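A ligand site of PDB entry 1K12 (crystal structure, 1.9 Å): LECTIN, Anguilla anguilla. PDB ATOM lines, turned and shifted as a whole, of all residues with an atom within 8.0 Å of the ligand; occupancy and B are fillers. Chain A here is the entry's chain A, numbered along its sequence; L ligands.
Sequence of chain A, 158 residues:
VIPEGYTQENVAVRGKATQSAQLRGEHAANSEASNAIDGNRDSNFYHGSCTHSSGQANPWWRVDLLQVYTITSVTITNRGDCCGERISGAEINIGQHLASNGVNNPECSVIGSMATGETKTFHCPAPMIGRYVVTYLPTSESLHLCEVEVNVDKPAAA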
ATOM      1  N   LEU A  23     -10.697  -5.398   1.516  1.00  0.00           N
ATOM      2  CA  LEU A  23     -11.577  -4.469   2.228  1.00  0.00           C
ATOM      3  C   LEU A  23     -12.511  -3.845   1.199  1.00  0.00           C
ATOM      4  O   LEU A  23     -12.042  -3.373   0.144  1.00  0.00           O
ATOM      5  CB  LEU A  23     -10.784  -3.358   2.910  1.00  0.00           C
ATOM      6  CG  LEU A  23     -11.618  -2.226   3.522  1.00  0.00           C
ATOM      7  CD1 LEU A  23     -12.418  -2.743   4.709  1.00  0.00           C
ATOM      8  CD2 LEU A  23     -10.708  -1.082   3.946  1.00  0.00           C
ATOM      9  N   ARG A  24     -13.808  -3.827   1.491  1.00  0.00           N
ATOM     10  CA  ARG A  24     -14.761  -3.224   0.574  1.00  0.00           C
ATOM     11  C   ARG A  24     -15.239  -1.907   1.094  1.00  0.00           C
ATOM     12  O   ARG A  24     -15.016  -1.549   2.258  1.00  0.00           O
ATOM     13  CB  ARG A  24     -15.963  -4.137   0.375  1.00  0.00           C
ATOM     14  CG  ARG A  24     -15.623  -5.412  -0.350  1.00  0.00           C
ATOM     15  CD  ARG A  24     -16.856  -6.244  -0.498  1.00  0.00           C
ATOM     16  NE  ARG A  24     -17.879  -5.448  -1.159  1.00  0.00           N
ATOM     17  CZ  ARG A  24     -19.170  -5.761  -1.142  1.00  0.00           C
ATOM     18  NH1 ARG A  24     -19.569  -6.862  -0.500  1.00  0.00           N
ATOM     19  NH2 ARG A  24     -20.067  -4.975  -1.743  1.00  0.00           N
ATOM     20  N   GLU A  26     -15.798   2.324   1.163  1.00  0.00           N
ATOM     21  CA  GLU A  26     -15.128   3.610   1.113  1.00  0.00           C
ATOM     22  C   GLU A  26     -13.621   3.623   0.845  1.00  0.00           C
ATOM     23  O   GLU A  26     -13.149   4.405   0.024  1.00  0.00           O
ATOM     24  CB  GLU A  26     -15.418   4.353   2.420  1.00  0.00           C
ATOM     25  CG  GLU A  26     -14.951   5.773   2.432  1.00  0.00           C
ATOM     26  CD  GLU A  26     -15.245   6.462   3.746  1.00  0.00           C
ATOM     27  OE1 GLU A  26     -14.859   7.652   3.871  1.00  0.00           O
ATOM     28  OE2 GLU A  26     -15.847   5.815   4.625  1.00  0.00           O
ATOM     29  N   HIS A  27     -12.867   2.782   1.541  1.00  0.00           N
ATOM     30  CA  HIS A  27     -11.423   2.788   1.377  1.00  0.00           C
ATOM     31  C   HIS A  27     -10.916   1.618   0.603  1.00  0.00           C
ATOM     32  O   HIS A  27      -9.713   1.359   0.607  1.00  0.00           O
ATOM     33  CB  HIS A  27     -10.744   2.809   2.757  1.00  0.00           C
ATOM     34  CG  HIS A  27     -11.244   3.896   3.646  1.00  0.00           C
ATOM     35  ND1 HIS A  27     -11.166   5.232   3.307  1.00  0.00           N
ATOM     36  CD2 HIS A  27     -11.868   3.853   4.845  1.00  0.00           C
ATOM     37  CE1 HIS A  27     -11.733   5.967   4.247  1.00  0.00           C
ATOM     38  NE2 HIS A  27     -12.168   5.145   5.196  1.00  0.00           N
ATOM     39  N   ALA A  28     -11.817   0.915  -0.066  1.00  0.00           N
ATOM     40  CA  ALA A  28     -11.465  -0.256  -0.859  1.00  0.00           C
ATOM     41  C   ALA A  28     -10.334  -0.003  -1.888  1.00  0.00           C
ATOM     42  O   ALA A  28      -9.533  -0.893  -2.157  1.00  0.00           O
ATOM     43  CB  ALA A  28     -12.705  -0.785  -1.567  1.00  0.00           C
ATOM     44  N   ASN A  30      -7.639   1.736  -1.619  1.00  0.00           N
ATOM     45  CA  ASN A  30      -6.312   1.832  -1.002  1.00  0.00           C
ATOM     46  C   ASN A  30      -5.882   0.466  -0.469  1.00  0.00           C
ATOM     47  O   ASN A  30      -4.818   0.348   0.108  1.00  0.00           O
ATOM     48  CB  ASN A  30      -6.326   2.793   0.206  1.00  0.00           C
ATOM     49  CG  ASN A  30      -6.674   4.247  -0.151  1.00  0.00           C
ATOM     50  OD1 ASN A  30      -6.152   4.835  -1.116  1.00  0.00           O
ATOM     51  ND2 ASN A  30      -7.533   4.852   0.672  1.00  0.00           N
ATOM     52  N   SER A  31      -6.708  -0.557  -0.664  1.00  0.00           N
ATOM     53  CA  SER A  31      -6.493  -1.888  -0.076  1.00  0.00           C
ATOM     54  C   SER A  31      -5.887  -3.061  -0.840  1.00  0.00           C
ATOM     55  O   SER A  31      -5.761  -4.137  -0.273  1.00  0.00           O
ATOM     56  CB  SER A  31      -7.835  -2.363   0.480  1.00  0.00           C
ATOM     57  OG  SER A  31      -8.395  -1.391   1.357  1.00  0.00           O
ATOM     58  N   PHE A  45      -1.878   4.199   5.915  1.00  0.00           N
ATOM     59  CA  PHE A  45      -2.794   3.485   5.026  1.00  0.00           C
ATOM     60  C   PHE A  45      -3.413   4.397   3.961  1.00  0.00           C
ATOM     61  O   PHE A  45      -3.626   3.986   2.807  1.00  0.00           O
ATOM     62  CB  PHE A  45      -3.907   2.828   5.862  1.00  0.00           C
ATOM     63  CG  PHE A  45      -5.007   2.204   5.027  1.00  0.00           C
ATOM     64  CD1 PHE A  45      -4.809   0.992   4.377  1.00  0.00           C
ATOM     65  CD2 PHE A  45      -6.236   2.866   4.872  1.00  0.00           C
ATOM     66  CE1 PHE A  45      -5.824   0.432   3.566  1.00  0.00           C
ATOM     67  CE2 PHE A  45      -7.252   2.307   4.061  1.00  0.00           C
ATOM     68  CZ  PHE A  45      -7.038   1.085   3.405  1.00  0.00           C
ATOM     69  N   TYR A  46      -3.689   5.637   4.324  1.00  0.00           N
ATOM     70  CA  TYR A  46      -4.303   6.559   3.385  1.00  0.00           C
ATOM     71  C   TYR A  46      -3.471   7.027   2.200  1.00  0.00           C
ATOM     72  O   TYR A  46      -3.989   7.703   1.317  1.00  0.00           O
ATOM     73  CB  TYR A  46      -4.922   7.736   4.140  1.00  0.00           C
ATOM     74  CG  TYR A  46      -6.056   7.249   5.011  1.00  0.00           C
ATOM     75  CD1 TYR A  46      -5.843   6.962   6.354  1.00  0.00           C
ATOM     76  CD2 TYR A  46      -7.320   7.010   4.464  1.00  0.00           C
ATOM     77  CE1 TYR A  46      -6.865   6.443   7.147  1.00  0.00           C
ATOM     78  CE2 TYR A  46      -8.346   6.498   5.237  1.00  0.00           C
ATOM     79  CZ  TYR A  46      -8.112   6.224   6.580  1.00  0.00           C
ATOM     80  OH  TYR A  46      -9.154   5.756   7.374  1.00  0.00           O
ATOM     81  N   THR A  51      -1.985  -3.044   2.294  1.00  0.00           N
ATOM     82  CA  THR A  51      -3.080  -3.949   1.944  1.00  0.00           C
ATOM     83  C   THR A  51      -4.099  -3.873   3.078  1.00  0.00           C
ATOM     84  O   THR A  51      -3.814  -3.352   4.149  1.00  0.00           O
ATOM     85  CB  THR A  51      -2.604  -5.415   1.848  1.00  0.00           C
ATOM     86  OG1 THR A  51      -2.327  -5.910   3.169  1.00  0.00           O
ATOM     87  CG2 THR A  51      -1.353  -5.522   0.991  1.00  0.00           C
ATOM     88  N   HIS A  52      -5.297  -4.382   2.837  1.00  0.00           N
ATOM     89  CA  HIS A  52      -6.314  -4.393   3.885  1.00  0.00           C
ATOM     90  C   HIS A  52      -7.331  -5.476   3.539  1.00  0.00           C
ATOM     91  O   HIS A  52      -7.922  -5.473   2.451  1.00  0.00           O
ATOM     92  CB  HIS A  52      -6.980  -3.003   3.986  1.00  0.00           C
ATOM     93  CG  HIS A  52      -7.718  -2.760   5.280  1.00  0.00           C
ATOM     94  ND1 HIS A  52      -8.659  -3.619   5.785  1.00  0.00           N
ATOM     95  CD2 HIS A  52      -7.675  -1.708   6.139  1.00  0.00           C
ATOM     96  CE1 HIS A  52      -9.174  -3.111   6.895  1.00  0.00           C
ATOM     97  NE2 HIS A  52      -8.592  -1.950   7.136  1.00  0.00           N
ATOM     98  N   SER A  53      -7.509  -6.441   4.452  1.00  0.00           N
ATOM     99  CA  SER A  53      -8.451  -7.526   4.244  1.00  0.00           C
ATOM    100  C   SER A  53      -9.894  -7.058   4.543  1.00  0.00           C
ATOM    101  O   SER A  53     -10.100  -5.960   5.057  1.00  0.00           O
ATOM    102  CB  SER A  53      -8.063  -8.754   5.097  1.00  0.00           C
ATOM    103  OG  SER A  53      -8.143  -8.473   6.487  1.00  0.00           O
ATOM    104  N   GLY A  55     -12.144  -7.893   6.758  1.00  0.00           N
ATOM    105  CA  GLY A  55     -12.568  -7.708   8.132  1.00  0.00           C
ATOM    106  C   GLY A  55     -13.171  -9.012   8.646  1.00  0.00           C
ATOM    107  O   GLY A  55     -13.417  -9.176   9.841  1.00  0.00           O
ATOM    108  N   ARG A  79       0.771  -1.364   9.955  1.00  0.00           N
ATOM    109  CA  ARG A  79       0.067  -0.100   9.698  1.00  0.00           C
ATOM    110  C   ARG A  79       0.451   0.961  10.736  1.00  0.00           C
ATOM    111  O   ARG A  79       0.547   0.672  11.932  1.00  0.00           O
ATOM    112  CB  ARG A  79      -1.443  -0.312   9.721  1.00  0.00           C
ATOM    113  CG  ARG A  79      -2.242   0.936   9.400  1.00  0.00           C
ATOM    114  CD  ARG A  79      -3.719   0.623   9.408  1.00  0.00           C
ATOM    115  NE  ARG A  79      -4.550   1.786   9.103  1.00  0.00           N
ATOM    116  CZ  ARG A  79      -5.874   1.751   8.983  1.00  0.00           C
ATOM    117  NH1 ARG A  79      -6.548   0.615   9.144  1.00  0.00           N
ATOM    118  NH2 ARG A  79      -6.531   2.871   8.689  1.00  0.00           N
ATOM    119  N   ASP A  81      -1.009   4.652  10.690  1.00  0.00           N
ATOM    120  CA  ASP A  81      -1.966   5.708  11.028  1.00  0.00           C
ATOM    121  C   ASP A  81      -2.870   5.333  12.204  1.00  0.00           C
ATOM    122  O   ASP A  81      -3.396   6.203  12.908  1.00  0.00           O
ATOM    123  CB  ASP A  81      -2.797   6.134   9.806  1.00  0.00           C
ATOM    124  CG  ASP A  81      -3.592   4.999   9.221  1.00  0.00           C
ATOM    125  OD1 ASP A  81      -4.837   5.094   9.204  1.00  0.00           O
ATOM    126  OD2 ASP A  81      -2.966   4.012   8.771  1.00  0.00           O
ATOM    127  N   CYS A  82      -3.062   4.036  12.405  1.00  0.00           N
ATOM    128  CA  CYS A  82      -3.866   3.506  13.503  1.00  0.00           C
ATOM    129  C   CYS A  82      -3.743   2.001  13.503  1.00  0.00           C
ATOM    130  O   CYS A  82      -2.982   1.401  12.738  1.00  0.00           O
ATOM    131  CB  CYS A  82      -5.375   3.779  13.316  1.00  0.00           C
ATOM    132  SG  CYS A  82      -6.244   2.633  12.163  1.00  0.00           S
ATOM    133  N   CYS A  83      -4.491   1.424  14.436  1.00  0.00           N
ATOM    134  CA  CYS A  83      -4.700  -0.006  14.511  1.00  0.00           C
ATOM    135  C   CYS A  83      -3.489  -0.942  14.462  1.00  0.00           C
ATOM    136  O   CYS A  83      -3.575  -2.023  13.888  1.00  0.00           O
ATOM    137  CB  CYS A  83      -5.701  -0.277  13.381  1.00  0.00           C
ATOM    138  SG  CYS A  83      -6.984   1.058  13.259  1.00  0.00           S
ATOM    139  N   GLU A  85      -2.337  -2.824  16.651  1.00  0.00           N
ATOM    140  CA  GLU A  85      -2.519  -4.031  17.452  1.00  0.00           C
ATOM    141  C   GLU A  85      -3.186  -5.198  16.738  1.00  0.00           C
ATOM    142  O   GLU A  85      -3.109  -6.336  17.209  1.00  0.00           O
ATOM    143  CB  GLU A  85      -3.325  -3.683  18.721  1.00  0.00           C
ATOM    144  CG  GLU A  85      -4.831  -3.385  18.503  1.00  0.00           C
ATOM    145  CD  GLU A  85      -5.121  -2.033  17.845  1.00  0.00           C
ATOM    146  OE1 GLU A  85      -5.653  -2.021  16.706  1.00  0.00           O
ATOM    147  OE2 GLU A  85      -4.834  -0.978  18.474  1.00  0.00           O
ATOM    148  N   ARG A  86      -3.827  -4.923  15.609  1.00  0.00           N
ATOM    149  CA  ARG A  86      -4.551  -5.972  14.881  1.00  0.00           C
ATOM    150  C   ARG A  86      -3.701  -7.125  14.345  1.00  0.00           C
ATOM    151  O   ARG A  86      -4.198  -8.249  14.210  1.00  0.00           O
ATOM    152  CB  ARG A  86      -5.346  -5.338  13.720  1.00  0.00           C
ATOM    153  CG  ARG A  86      -6.385  -4.325  14.169  1.00  0.00           C
ATOM    154  CD  ARG A  86      -7.152  -3.797  12.987  1.00  0.00           C
ATOM    155  NE  ARG A  86      -8.284  -2.946  13.381  1.00  0.00           N
ATOM    156  CZ  ARG A  86      -8.900  -2.109  12.569  1.00  0.00           C
ATOM    157  NH1 ARG A  86      -8.508  -1.985  11.305  1.00  0.00           N
ATOM    158  NH2 ARG A  86      -9.914  -1.378  13.007  1.00  0.00           N
ATOM    159  N   GLU A 141      -9.533 -10.048  13.578  1.00  0.00           N
ATOM    160  CA  GLU A 141      -9.069  -8.727  13.220  1.00  0.00           C
ATOM    161  C   GLU A 141      -8.799  -8.541  11.731  1.00  0.00           C
ATOM    162  O   GLU A 141      -8.685  -9.516  10.969  1.00  0.00           O
ATOM    163  CB  GLU A 141      -7.809  -8.388  14.019  1.00  0.00           C
ATOM    164  CG  GLU A 141      -8.097  -8.219  15.487  1.00  0.00           C
ATOM    165  CD  GLU A 141      -9.118  -7.129  15.767  1.00  0.00           C
ATOM    166  OE1 GLU A 141      -9.719  -7.128  16.861  1.00  0.00           O
ATOM    167  OE2 GLU A 141      -9.335  -6.256  14.887  1.00  0.00           O
ATOM    168  N   SER A 142      -8.728  -7.287  11.309  1.00  0.00           N
ATOM    169  CA  SER A 142      -8.421  -6.977   9.916  1.00  0.00           C
ATOM    170  C   SER A 142      -6.919  -7.110   9.735  1.00  0.00           C
ATOM    171  O   SER A 142      -6.135  -6.699  10.617  1.00  0.00           O
ATOM    172  CB  SER A 142      -8.833  -5.558   9.575  1.00  0.00           C
ATOM    173  OG  SER A 142     -10.230  -5.411   9.689  1.00  0.00           O
ATOM    174  N   LEU A 143      -6.512  -7.668   8.610  1.00  0.00           N
ATOM    175  CA  LEU A 143      -5.099  -7.809   8.333  1.00  0.00           C
ATOM    176  C   LEU A 143      -4.673  -6.712   7.350  1.00  0.00           C
ATOM    177  O   LEU A 143      -5.192  -6.630   6.231  1.00  0.00           O
ATOM    178  CB  LEU A 143      -4.784  -9.194   7.748  1.00  0.00           C
ATOM    179  CG  LEU A 143      -3.364  -9.448   7.247  1.00  0.00           C
ATOM    180  CD1 LEU A 143      -2.364  -9.265   8.382  1.00  0.00           C
ATOM    181  CD2 LEU A 143      -3.292 -10.850   6.659  1.00  0.00           C
ATOM    182  N   HIS A 144      -3.798  -5.835   7.808  1.00  0.00           N
ATOM    183  CA  HIS A 144      -3.276  -4.778   6.948  1.00  0.00           C
ATOM    184  C   HIS A 144      -1.752  -4.741   7.042  1.00  0.00           C
ATOM    185  O   HIS A 144      -1.176  -4.506   8.105  1.00  0.00           O
ATOM    186  CB  HIS A 144      -3.930  -3.398   7.225  1.00  0.00           C
ATOM    187  CG  HIS A 144      -4.319  -3.126   8.650  1.00  0.00           C
ATOM    188  ND1 HIS A 144      -5.576  -2.661   8.994  1.00  0.00           N
ATOM    189  CD2 HIS A 144      -3.602  -3.139   9.798  1.00  0.00           C
ATOM    190  CE1 HIS A 144      -5.609  -2.387  10.292  1.00  0.00           C
ATOM    191  NE2 HIS A 144      -4.425  -2.670  10.799  1.00  0.00           N
HETATM  192  C1  LIG L   1      -9.657   2.921  10.336  1.00  0.00           C
HETATM  193  C2  LIG L   1     -10.120   1.640  11.056  1.00  0.00           C
HETATM  194  C3  LIG L   1     -11.108   0.872  10.191  1.00  0.00           C
HETATM  195  C4  LIG L   1     -10.455   0.573   8.828  1.00  0.00           C
HETATM  196  C5  LIG L   1     -10.052   1.914   8.177  1.00  0.00           C
HETATM  197  C6  LIG L   1      -9.388   1.755   6.815  1.00  0.00           C
HETATM  198  O1  LIG L   1     -10.711   3.814  10.186  1.00  0.00           O
HETATM  199  O2  LIG L   1     -10.733   1.979  12.300  1.00  0.00           O
HETATM  200  O3  LIG L   1     -11.476  -0.343  10.834  1.00  0.00           O
HETATM  201  O4  LIG L   1      -9.304  -0.244   9.015  1.00  0.00           O
HETATM  202  O5  LIG L   1      -9.121   2.614   9.030  1.00  0.00           O
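Merely in contact with the ligand: Phe 45 (3.5 Å), Tyr 46 (3.6 Å), His 27 (3.8 Å), Cys 83 (3.9 Å) and Cys 82 (3.9 Å).
Hydrophobic or aromatic side chains that line the ligand: His 27, Phe 45 and His 52.
Eight residues have an atom within 4 Å of the ligand: His 27, Phe 45, Tyr 46, His 52, Arg 79, Cys 82, Cys 83 and Arg 86.
A ring nitrogen (NE2) of His 144 sits at hydrogen-bond distance from the backbone carbonyl oxygen of Cys 83 (3.3 Å).
O of His 27 is in hydrogen-bond range of OG of Ser 31 (3.1 Å).
The guanidinium group (NH2) of Arg 79 lies close to the side-chain sulfur (SG) of Cys 82 (3.5 Å).
The backbone carbonyl oxygen (O) of Ser 31 sits at hydrogen-bond distance from the backbone NH (N) of His 52, 3.2 Å away.
SG of Cys 82 is disulfide-bonded to SG of Cys 83.
OD2 of Asp 81 is in hydrogen-bond range of N of Phe 45 (3.1 Å).
The guanidinium group (NH1) of Arg 79 sits close to a ring nitrogen (ND1) of His 144 (3.4 Å).
The backbone NH (N) of Leu 23 sits at hydrogen-bond distance from the backbone carbonyl oxygen (O) of His 52 (2.9 Å).
NH2 of Arg 86 lies within hydrogen-bond range of O3 of the ligand, at 2.9 Å.
The guanidinium group (NH2) of Arg 79 sits at hydrogen-bond distance from an oxygen (O5) of the ligand, at 2.6 Å.
A ring nitrogen (NE2) of His 52 lies within hydrogen-bond range of an oxygen (O4) of the ligand (2.6 Å).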
